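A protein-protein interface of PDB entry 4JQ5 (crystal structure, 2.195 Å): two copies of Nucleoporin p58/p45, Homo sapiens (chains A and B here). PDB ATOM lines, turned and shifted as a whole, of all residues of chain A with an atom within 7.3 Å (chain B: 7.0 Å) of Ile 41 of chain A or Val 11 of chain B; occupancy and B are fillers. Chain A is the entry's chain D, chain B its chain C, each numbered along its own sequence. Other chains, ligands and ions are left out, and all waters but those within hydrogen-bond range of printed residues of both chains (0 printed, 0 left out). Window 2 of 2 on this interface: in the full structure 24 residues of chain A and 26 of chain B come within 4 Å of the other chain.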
ATOM      1  N   HIS A  31     -31.394   9.012 -17.621  1.00  0.00           N
ATOM      2  CA  HIS A  31     -29.937   8.995 -17.645  1.00  0.00           C
ATOM      3  C   HIS A  31     -29.380   9.250 -16.249  1.00  0.00           C
ATOM      4  O   HIS A  31     -28.371   8.666 -15.858  1.00  0.00           O
ATOM      5  CB  HIS A  31     -29.412  10.051 -18.618  1.00  0.00           C
ATOM      6  CG  HIS A  31     -27.922  10.055 -18.761  1.00  0.00           C
ATOM      7  ND1 HIS A  31     -27.113   9.093 -18.193  1.00  0.00           N
ATOM      8  CD2 HIS A  31     -27.091  10.907 -19.408  1.00  0.00           C
ATOM      9  CE1 HIS A  31     -25.853   9.352 -18.484  1.00  0.00           C
ATOM     10  NE2 HIS A  31     -25.810  10.448 -19.221  1.00  0.00           N
ATOM     11  N   LEU A  32     -30.043  10.127 -15.502  1.00  0.00           N
ATOM     12  CA  LEU A  32     -29.624  10.437 -14.140  1.00  0.00           C
ATOM     13  C   LEU A  32     -29.931   9.275 -13.204  1.00  0.00           C
ATOM     14  O   LEU A  32     -29.181   9.007 -12.267  1.00  0.00           O
ATOM     15  CB  LEU A  32     -30.312  11.707 -13.643  1.00  0.00           C
ATOM     16  CG  LEU A  32     -29.928  12.990 -14.382  1.00  0.00           C
ATOM     17  CD1 LEU A  32     -30.752  14.162 -13.880  1.00  0.00           C
ATOM     18  CD2 LEU A  32     -28.442  13.281 -14.230  1.00  0.00           C
ATOM     19  N   ALA A  33     -31.039   8.588 -13.461  1.00  0.00           N
ATOM     20  CA  ALA A  33     -31.398   7.409 -12.683  1.00  0.00           C
ATOM     21  C   ALA A  33     -30.370   6.307 -12.914  1.00  0.00           C
ATOM     22  O   ALA A  33     -30.090   5.508 -12.019  1.00  0.00           O
ATOM     23  CB  ALA A  33     -32.788   6.929 -13.061  1.00  0.00           C
ATOM     24  N   THR A  34     -29.812   6.269 -14.119  1.00  0.00           N
ATOM     25  CA  THR A  34     -28.786   5.290 -14.461  1.00  0.00           C
ATOM     26  C   THR A  34     -27.474   5.582 -13.741  1.00  0.00           C
ATOM     27  O   THR A  34     -26.936   4.719 -13.047  1.00  0.00           O
ATOM     28  CB  THR A  34     -28.526   5.257 -15.978  1.00  0.00           C
ATOM     29  OG1 THR A  34     -29.681   4.745 -16.653  1.00  0.00           O
ATOM     30  CG2 THR A  34     -27.325   4.377 -16.299  1.00  0.00           C
ATOM     31  N   GLN A  35     -26.964   6.800 -13.901  1.00  0.00           N
ATOM     32  CA  GLN A  35     -25.699   7.182 -13.280  1.00  0.00           C
ATOM     33  C   GLN A  35     -25.858   7.541 -11.801  1.00  0.00           C
ATOM     34  O   GLN A  35     -25.004   8.215 -11.224  1.00  0.00           O
ATOM     35  CB  GLN A  35     -25.049   8.344 -14.037  1.00  0.00           C
ATOM     36  CG  GLN A  35     -24.372   7.929 -15.335  1.00  0.00           C
ATOM     37  CD  GLN A  35     -23.420   8.987 -15.862  1.00  0.00           C
ATOM     38  OE1 GLN A  35     -23.456  10.141 -15.433  1.00  0.00           O
ATOM     39  NE2 GLN A  35     -22.556   8.595 -16.791  1.00  0.00           N
ATOM     40  N   ALA A  36     -26.954   7.091 -11.195  1.00  0.00           N
ATOM     41  CA  ALA A  36     -27.146   7.224  -9.756  1.00  0.00           C
ATOM     42  C   ALA A  36     -26.909   5.876  -9.081  1.00  0.00           C
ATOM     43  O   ALA A  36     -26.350   5.809  -7.986  1.00  0.00           O
ATOM     44  CB  ALA A  36     -28.544   7.731  -9.454  1.00  0.00           C
ATOM     45  N   ASN A  37     -27.338   4.805  -9.745  1.00  0.00           N
ATOM     46  CA  ASN A  37     -27.141   3.452  -9.234  1.00  0.00           C
ATOM     47  C   ASN A  37     -25.761   2.897  -9.592  1.00  0.00           C
ATOM     48  O   ASN A  37     -25.268   1.977  -8.941  1.00  0.00           O
ATOM     49  CB  ASN A  37     -28.242   2.520  -9.754  1.00  0.00           C
ATOM     50  CG  ASN A  37     -29.622   2.916  -9.261  1.00  0.00           C
ATOM     51  OD1 ASN A  37     -29.757   3.611  -8.254  1.00  0.00           O
ATOM     52  ND2 ASN A  37     -30.657   2.471  -9.967  1.00  0.00           N
ATOM     53  N   ASN A  38     -25.144   3.465 -10.625  1.00  0.00           N
ATOM     54  CA  ASN A  38     -23.790   3.086 -11.019  1.00  0.00           C
ATOM     55  C   ASN A  38     -22.789   3.668 -10.026  1.00  0.00           C
ATOM     56  O   ASN A  38     -22.290   2.966  -9.146  1.00  0.00           O
ATOM     57  CB  ASN A  38     -23.482   3.578 -12.438  1.00  0.00           C
ATOM     58  CG  ASN A  38     -24.203   2.773 -13.507  1.00  0.00           C
ATOM     59  OD1 ASN A  38     -25.201   2.108 -13.233  1.00  0.00           O
ATOM     60  ND2 ASN A  38     -23.698   2.834 -14.738  1.00  0.00           N
ATOM     61  N   SER A  39     -22.507   4.960 -10.167  1.00  0.00           N
ATOM     62  CA  SER A  39     -21.654   5.671  -9.225  1.00  0.00           C
ATOM     63  C   SER A  39     -22.529   6.648  -8.447  1.00  0.00           C
ATOM     64  O   SER A  39     -23.592   6.271  -7.952  1.00  0.00           O
ATOM     65  CB  SER A  39     -20.534   6.410  -9.961  1.00  0.00           C
ATOM     66  OG  SER A  39     -21.045   7.494 -10.715  1.00  0.00           O
ATOM     67  N   HIS A  40     -22.090   7.897  -8.339  1.00  0.00           N
ATOM     68  CA  HIS A  40     -22.921   8.942  -7.758  1.00  0.00           C
ATOM     69  C   HIS A  40     -22.966  10.131  -8.706  1.00  0.00           C
ATOM     70  O   HIS A  40     -21.945  10.516  -9.276  1.00  0.00           O
ATOM     71  CB  HIS A  40     -22.383   9.369  -6.390  1.00  0.00           C
ATOM     72  CG  HIS A  40     -21.073  10.091  -6.452  1.00  0.00           C
ATOM     73  ND1 HIS A  40     -19.863   9.462  -6.254  1.00  0.00           N
ATOM     74  CD2 HIS A  40     -20.785  11.394  -6.690  1.00  0.00           C
ATOM     75  CE1 HIS A  40     -18.887  10.343  -6.365  1.00  0.00           C
ATOM     76  NE2 HIS A  40     -19.419  11.524  -6.631  1.00  0.00           N
ATOM     77  N   ILE A  41     -24.153  10.701  -8.885  1.00  0.00           N
ATOM     78  CA  ILE A  41     -24.315  11.855  -9.760  1.00  0.00           C
ATOM     79  C   ILE A  41     -23.384  12.969  -9.297  1.00  0.00           C
ATOM     80  O   ILE A  41     -23.272  13.236  -8.101  1.00  0.00           O
ATOM     81  CB  ILE A  41     -25.769  12.360  -9.775  1.00  0.00           C
ATOM     82  CG1 ILE A  41     -26.701  11.266 -10.304  1.00  0.00           C
ATOM     83  CG2 ILE A  41     -25.887  13.612 -10.633  1.00  0.00           C
ATOM     84  CD1 ILE A  41     -28.168  11.635 -10.276  1.00  0.00           C
ATOM     85  N   THR A  42     -22.715  13.611 -10.249  1.00  0.00           N
ATOM     86  CA  THR A  42     -21.706  14.616  -9.937  1.00  0.00           C
ATOM     87  C   THR A  42     -22.138  16.004 -10.395  1.00  0.00           C
ATOM     88  O   THR A  42     -23.057  16.136 -11.202  1.00  0.00           O
ATOM     89  CB  THR A  42     -20.372  14.278 -10.619  1.00  0.00           C
ATOM     90  OG1 THR A  42     -20.490  14.473 -12.033  1.00  0.00           O
ATOM     91  CG2 THR A  42     -19.980  12.838 -10.340  1.00  0.00           C
ATOM     92  N   PRO A  43     -21.475  17.049  -9.875  1.00  0.00           N
ATOM     93  CA  PRO A  43     -21.738  18.426 -10.308  1.00  0.00           C
ATOM     94  C   PRO A  43     -21.568  18.597 -11.815  1.00  0.00           C
ATOM     95  O   PRO A  43     -22.249  19.423 -12.425  1.00  0.00           O
ATOM     96  CB  PRO A  43     -20.677  19.233  -9.560  1.00  0.00           C
ATOM     97  CG  PRO A  43     -20.384  18.432  -8.349  1.00  0.00           C
ATOM     98  CD  PRO A  43     -20.494  17.000  -8.776  1.00  0.00           C
ATOM     99  N   GLN A  44     -20.656  17.827 -12.400  1.00  0.00           N
ATOM    100  CA  GLN A  44     -20.470  17.817 -13.845  1.00  0.00           C
ATOM    101  C   GLN A  44     -21.757  17.365 -14.523  1.00  0.00           C
ATOM    102  O   GLN A  44     -22.227  17.989 -15.477  1.00  0.00           O
ATOM    103  CB  GLN A  44     -19.329  16.871 -14.225  1.00  0.00           C
ATOM    104  CG  GLN A  44     -19.222  16.576 -15.716  1.00  0.00           C
ATOM    105  CD  GLN A  44     -19.086  15.092 -16.008  1.00  0.00           C
ATOM    106  OE1 GLN A  44     -20.048  14.433 -16.399  1.00  0.00           O
ATOM    107  NE2 GLN A  44     -17.884  14.561 -15.818  1.00  0.00           N
ATOM    108  N   ASP A  45     -22.318  16.268 -14.025  1.00  0.00           N
ATOM    109  CA  ASP A  45     -23.558  15.735 -14.568  1.00  0.00           C
ATOM    110  C   ASP A  45     -24.679  16.773 -14.489  1.00  0.00           C
ATOM    111  O   ASP A  45     -25.354  17.052 -15.484  1.00  0.00           O
ATOM    112  CB  ASP A  45     -23.981  14.469 -13.813  1.00  0.00           C
ATOM    113  CG  ASP A  45     -22.914  13.386 -13.830  1.00  0.00           C
ATOM    114  OD1 ASP A  45     -22.030  13.420 -14.712  1.00  0.00           O
ATOM    115  OD2 ASP A  45     -22.967  12.493 -12.956  1.00  0.00           O
ATOM    116  N   LEU A  46     -24.877  17.334 -13.300  1.00  0.00           N
ATOM    117  CA  LEU A  46     -25.942  18.307 -13.080  1.00  0.00           C
ATOM    118  C   LEU A  46     -25.815  19.489 -14.038  1.00  0.00           C
ATOM    119  O   LEU A  46     -26.812  19.978 -14.576  1.00  0.00           O
ATOM    120  CB  LEU A  46     -25.917  18.813 -11.636  1.00  0.00           C
ATOM    121  CG  LEU A  46     -27.277  18.855 -10.936  1.00  0.00           C
ATOM    122  CD1 LEU A  46     -27.118  19.408  -9.533  1.00  0.00           C
ATOM    123  CD2 LEU A  46     -28.287  19.678 -11.725  1.00  0.00           C
ATOM    124  N   ASP B   5     -23.686  15.171   1.063  1.00  0.00           N
ATOM    125  CA  ASP B   5     -25.084  15.182   1.481  1.00  0.00           C
ATOM    126  C   ASP B   5     -25.824  16.383   0.892  1.00  0.00           C
ATOM    127  O   ASP B   5     -26.896  16.234   0.303  1.00  0.00           O
ATOM    128  CB  ASP B   5     -25.188  15.205   3.008  1.00  0.00           C
ATOM    129  CG  ASP B   5     -24.678  13.928   3.649  1.00  0.00           C
ATOM    130  OD1 ASP B   5     -23.853  13.231   3.022  1.00  0.00           O
ATOM    131  OD2 ASP B   5     -25.102  13.624   4.784  1.00  0.00           O
ATOM    132  N   TYR B   6     -25.251  17.572   1.058  1.00  0.00           N
ATOM    133  CA  TYR B   6     -25.836  18.786   0.498  1.00  0.00           C
ATOM    134  C   TYR B   6     -26.135  18.591  -0.984  1.00  0.00           C
ATOM    135  O   TYR B   6     -27.259  18.810  -1.438  1.00  0.00           O
ATOM    136  CB  TYR B   6     -24.897  19.983   0.681  1.00  0.00           C
ATOM    137  CG  TYR B   6     -24.755  20.455   2.112  1.00  0.00           C
ATOM    138  CD1 TYR B   6     -25.825  21.033   2.780  1.00  0.00           C
ATOM    139  CD2 TYR B   6     -23.548  20.338   2.789  1.00  0.00           C
ATOM    140  CE1 TYR B   6     -25.702  21.472   4.087  1.00  0.00           C
ATOM    141  CE2 TYR B   6     -23.414  20.775   4.095  1.00  0.00           C
ATOM    142  CZ  TYR B   6     -24.494  21.342   4.739  1.00  0.00           C
ATOM    143  OH  TYR B   6     -24.370  21.777   6.039  1.00  0.00           O
ATOM    144  N   PHE B   7     -25.120  18.173  -1.732  1.00  0.00           N
ATOM    145  CA  PHE B   7     -25.258  17.985  -3.170  1.00  0.00           C
ATOM    146  C   PHE B   7     -26.277  16.898  -3.496  1.00  0.00           C
ATOM    147  O   PHE B   7     -26.984  16.983  -4.496  1.00  0.00           O
ATOM    148  CB  PHE B   7     -23.910  17.640  -3.799  1.00  0.00           C
ATOM    149  CG  PHE B   7     -23.949  17.557  -5.296  1.00  0.00           C
ATOM    150  CD1 PHE B   7     -23.846  18.703  -6.068  1.00  0.00           C
ATOM    151  CD2 PHE B   7     -24.095  16.337  -5.934  1.00  0.00           C
ATOM    152  CE1 PHE B   7     -23.885  18.633  -7.447  1.00  0.00           C
ATOM    153  CE2 PHE B   7     -24.134  16.260  -7.312  1.00  0.00           C
ATOM    154  CZ  PHE B   7     -24.029  17.410  -8.070  1.00  0.00           C
ATOM    155  N   ARG B   8     -26.342  15.876  -2.649  1.00  0.00           N
ATOM    156  CA  ARG B   8     -27.297  14.790  -2.831  1.00  0.00           C
ATOM    157  C   ARG B   8     -28.709  15.359  -2.841  1.00  0.00           C
ATOM    158  O   ARG B   8     -29.533  15.009  -3.691  1.00  0.00           O
ATOM    159  CB  ARG B   8     -27.151  13.770  -1.701  1.00  0.00           C
ATOM    160  CG  ARG B   8     -27.746  12.407  -1.995  1.00  0.00           C
ATOM    161  CD  ARG B   8     -27.386  11.416  -0.897  1.00  0.00           C
ATOM    162  NE  ARG B   8     -27.787  10.049  -1.222  1.00  0.00           N
ATOM    163  CZ  ARG B   8     -27.060   9.199  -1.942  1.00  0.00           C
ATOM    164  NH1 ARG B   8     -25.881   9.563  -2.432  1.00  0.00           N
ATOM    165  NH2 ARG B   8     -27.515   7.977  -2.179  1.00  0.00           N
ATOM    166  N   ILE B   9     -28.981  16.247  -1.891  1.00  0.00           N
ATOM    167  CA  ILE B   9     -30.277  16.906  -1.810  1.00  0.00           C
ATOM    168  C   ILE B   9     -30.524  17.789  -3.030  1.00  0.00           C
ATOM    169  O   ILE B   9     -31.632  17.820  -3.565  1.00  0.00           O
ATOM    170  CB  ILE B   9     -30.387  17.750  -0.532  1.00  0.00           C
ATOM    171  CG1 ILE B   9     -30.391  16.830   0.689  1.00  0.00           C
ATOM    172  CG2 ILE B   9     -31.648  18.604  -0.559  1.00  0.00           C
ATOM    173  CD1 ILE B   9     -30.394  17.560   2.000  1.00  0.00           C
ATOM    174  N   LEU B  10     -29.494  18.507  -3.465  1.00  0.00           N
ATOM    175  CA  LEU B  10     -29.600  19.323  -4.670  1.00  0.00           C
ATOM    176  C   LEU B  10     -29.937  18.457  -5.880  1.00  0.00           C
ATOM    177  O   LEU B  10     -30.667  18.879  -6.780  1.00  0.00           O
ATOM    178  CB  LEU B  10     -28.294  20.077  -4.927  1.00  0.00           C
ATOM    179  CG  LEU B  10     -27.918  21.147  -3.901  1.00  0.00           C
ATOM    180  CD1 LEU B  10     -26.592  21.789  -4.273  1.00  0.00           C
ATOM    181  CD2 LEU B  10     -29.010  22.200  -3.794  1.00  0.00           C
ATOM    182  N   VAL B  11     -29.410  17.238  -5.889  1.00  0.00           N
ATOM    183  CA  VAL B  11     -29.566  16.348  -7.029  1.00  0.00           C
ATOM    184  C   VAL B  11     -30.983  15.806  -7.093  1.00  0.00           C
ATOM    185  O   VAL B  11     -31.583  15.763  -8.164  1.00  0.00           O
ATOM    186  CB  VAL B  11     -28.574  15.173  -6.972  1.00  0.00           C
ATOM    187  CG1 VAL B  11     -29.073  14.000  -7.809  1.00  0.00           C
ATOM    188  CG2 VAL B  11     -27.202  15.623  -7.445  1.00  0.00           C
ATOM    189  N   GLN B  12     -31.521  15.385  -5.955  1.00  0.00           N
ATOM    190  CA  GLN B  12     -32.883  14.872  -5.942  1.00  0.00           C
ATOM    191  C   GLN B  12     -33.891  16.006  -6.105  1.00  0.00           C
ATOM    192  O   GLN B  12     -35.023  15.777  -6.531  1.00  0.00           O
ATOM    193  CB  GLN B  12     -33.177  14.069  -4.672  1.00  0.00           C
ATOM    194  CG  GLN B  12     -33.554  14.905  -3.459  1.00  0.00           C
ATOM    195  CD  GLN B  12     -34.043  14.073  -2.279  1.00  0.00           C
ATOM    196  OE1 GLN B  12     -34.253  14.602  -1.187  1.00  0.00           O
ATOM    197  NE2 GLN B  12     -34.235  12.770  -2.491  1.00  0.00           N
ATOM    198  N   GLN B  13     -33.487  17.226  -5.766  1.00  0.00           N
ATOM    199  CA  GLN B  13     -34.333  18.385  -6.014  1.00  0.00           C
ATOM    200  C   GLN B  13     -34.430  18.641  -7.511  1.00  0.00           C
ATOM    201  O   GLN B  13     -35.505  18.939  -8.028  1.00  0.00           O
ATOM    202  CB  GLN B  13     -33.797  19.634  -5.316  1.00  0.00           C
ATOM    203  CG  GLN B  13     -34.154  20.913  -6.057  1.00  0.00           C
ATOM    204  CD  GLN B  13     -34.223  22.130  -5.156  1.00  0.00           C
ATOM    205  OE1 GLN B  13     -33.342  22.361  -4.327  1.00  0.00           O
ATOM    206  NE2 GLN B  13     -35.282  22.915  -5.317  1.00  0.00           N
ATOM    207  N   PHE B  14     -33.300  18.537  -8.201  1.00  0.00           N
ATOM    208  CA  PHE B  14     -33.277  18.693  -9.648  1.00  0.00           C
ATOM    209  C   PHE B  14     -34.168  17.653 -10.322  1.00  0.00           C
ATOM    210  O   PHE B  14     -35.057  17.997 -11.100  1.00  0.00           O
ATOM    211  CB  PHE B  14     -31.851  18.570 -10.181  1.00  0.00           C
ATOM    212  CG  PHE B  14     -31.764  18.600 -11.679  1.00  0.00           C
ATOM    213  CD1 PHE B  14     -31.664  19.804 -12.356  1.00  0.00           C
ATOM    214  CD2 PHE B  14     -31.791  17.425 -12.411  1.00  0.00           C
ATOM    215  CE1 PHE B  14     -31.589  19.833 -13.736  1.00  0.00           C
ATOM    216  CE2 PHE B  14     -31.715  17.451 -13.790  1.00  0.00           C
ATOM    217  CZ  PHE B  14     -31.613  18.657 -14.453  1.00  0.00           C
ATOM    218  N   GLU B  15     -33.920  16.382 -10.018  1.00  0.00           N
ATOM    219  CA  GLU B  15     -34.668  15.282 -10.616  1.00  0.00           C
ATOM    220  C   GLU B  15     -36.164  15.450 -10.390  1.00  0.00           C
ATOM    221  O   GLU B  15     -36.963  15.323 -11.318  1.00  0.00           O
ATOM    222  CB  GLU B  15     -34.213  13.947 -10.021  1.00  0.00           C
ATOM    223  CG  GLU B  15     -32.780  13.570 -10.356  1.00  0.00           C
ATOM    224  CD  GLU B  15     -32.341  12.292  -9.670  1.00  0.00           C
ATOM    225  OE1 GLU B  15     -33.160  11.697  -8.936  1.00  0.00           O
ATOM    226  OE2 GLU B  15     -31.176  11.882  -9.862  1.00  0.00           O
ATOM    227  N   VAL B  16     -36.533  15.735  -9.148  1.00  0.00           N
ATOM    228  CA  VAL B  16     -37.932  15.851  -8.762  1.00  0.00           C
ATOM    229  C   VAL B  16     -38.612  17.051  -9.419  1.00  0.00           C
ATOM    230  O   VAL B  16     -39.800  17.002  -9.743  1.00  0.00           O
ATOM    231  CB  VAL B  16     -38.056  15.959  -7.234  1.00  0.00           C
ATOM    232  CG1 VAL B  16     -39.394  16.532  -6.846  1.00  0.00           C
ATOM    233  CG2 VAL B  16     -37.843  14.599  -6.597  1.00  0.00           C
ATOM    234  N   GLN B  17     -37.859  18.127  -9.612  1.00  0.00           N
ATOM    235  CA  GLN B  17     -38.390  19.313 -10.269  1.00  0.00           C
ATOM    236  C   GLN B  17     -38.648  18.988 -11.732  1.00  0.00           C
ATOM    237  O   GLN B  17     -39.616  19.457 -12.330  1.00  0.00           O
ATOM    238  CB  GLN B  17     -37.400  20.471 -10.166  1.00  0.00           C
ATOM    239  CG  GLN B  17     -38.054  21.831 -10.074  1.00  0.00           C
ATOM    240  CD  GLN B  17     -39.035  21.938  -8.921  1.00  0.00           C
ATOM    241  OE1 GLN B  17     -40.067  22.601  -9.034  1.00  0.00           O
ATOM    242  NE2 GLN B  17     -38.721  21.289  -7.804  1.00  0.00           N
ATOM    243  N   ILE B  67     -30.938  26.061  -7.920  1.00  0.00           N
ATOM    244  CA  ILE B  67     -29.997  24.986  -7.606  1.00  0.00           C
ATOM    245  C   ILE B  67     -28.604  25.284  -8.176  1.00  0.00           C
ATOM    246  O   ILE B  67     -27.585  24.871  -7.610  1.00  0.00           O
ATOM    247  CB  ILE B  67     -30.488  23.601  -8.097  1.00  0.00           C
ATOM    248  CG1 ILE B  67     -30.258  23.439  -9.599  1.00  0.00           C
ATOM    249  CG2 ILE B  67     -31.952  23.373  -7.726  1.00  0.00           C
ATOM    250  CD1 ILE B  67     -29.028  22.622  -9.935  1.00  0.00           C
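CE2 of Phe 14 of chain B touches CD1 of Leu 32 of chain A (3.4 Å). Leu 32 of chain A touches Glu 15 of chain B. Ile 41 of chain A touches Phe 7 of chain B (O to CE2, 3.2 Å). Ile 41 of chain A touches Val 11 of chain B (CD1 to CG1, 3.5 Å). Ile 41 of chain A touches Glu 15 of chain B (CD1 to OE2, 3.0 Å). Phe 7 of chain B touches Thr 42 of chain A (CZ to C, 3.3 Å). Phe 7 of chain B touches Pro 43 of chain A (CZ to N, 3.1 Å). CE1 of Phe 7 of chain B touches CD1 of Leu 46 of chain A, 3.9 Å away. CD1 of Phe 14 of chain B touches CD2 of Leu 46 of chain A (3.4 Å). Ile 67 of chain B touches Leu 46 of chain A.
No position is printed for both chains.
The side-chain hydroxyl (OG1) of Thr 42 of chain A sits close to the backbone NH (N) of Gln 44 of chain A (3.4 Å). OD2 of Asp 45 of chain A sits at hydrogen-bond distance from N of Thr 42 of chain A (2.9 Å).
Ser 39 of chain A touches none of the printed residues of chain B. Of the printed residues of chain B, Ile 41 of chain A touches Phe 7, Val 11 and Glu 15. Printed residues of chain B within 4 Å of Thr 42 of chain A: Phe 7. Of the printed residues of chain B, Pro 43 of chain A touches Phe 7. Printed residues of chain B within 4 Å of Leu 46 of chain A: Phe 7, Phe 14 and Ile 67. Val 11 of chain B touches one residue of chain A. Printed residues of chain A within 4 Å of Glu 15 of chain B: Leu 32 and Ile 41. Of the printed residues of chain A, Ile 67 of chain B touches Leu 46. The nearest printed residue of chain B that does not touch Pro 43 of chain A is Val 11 of chain B (6.4 Å).
Hydrophobic or aromatic side chains of chain B that line the printed part of chain A: Phe 7, Val 11, Phe 14 and Ile 67. Printed residues of chain A that touch a printed residue of chain B: Leu 32, Ile 41, Thr 42, Pro 43 and Leu 46. Among the printed residues, 10 pairs touch across the chains.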
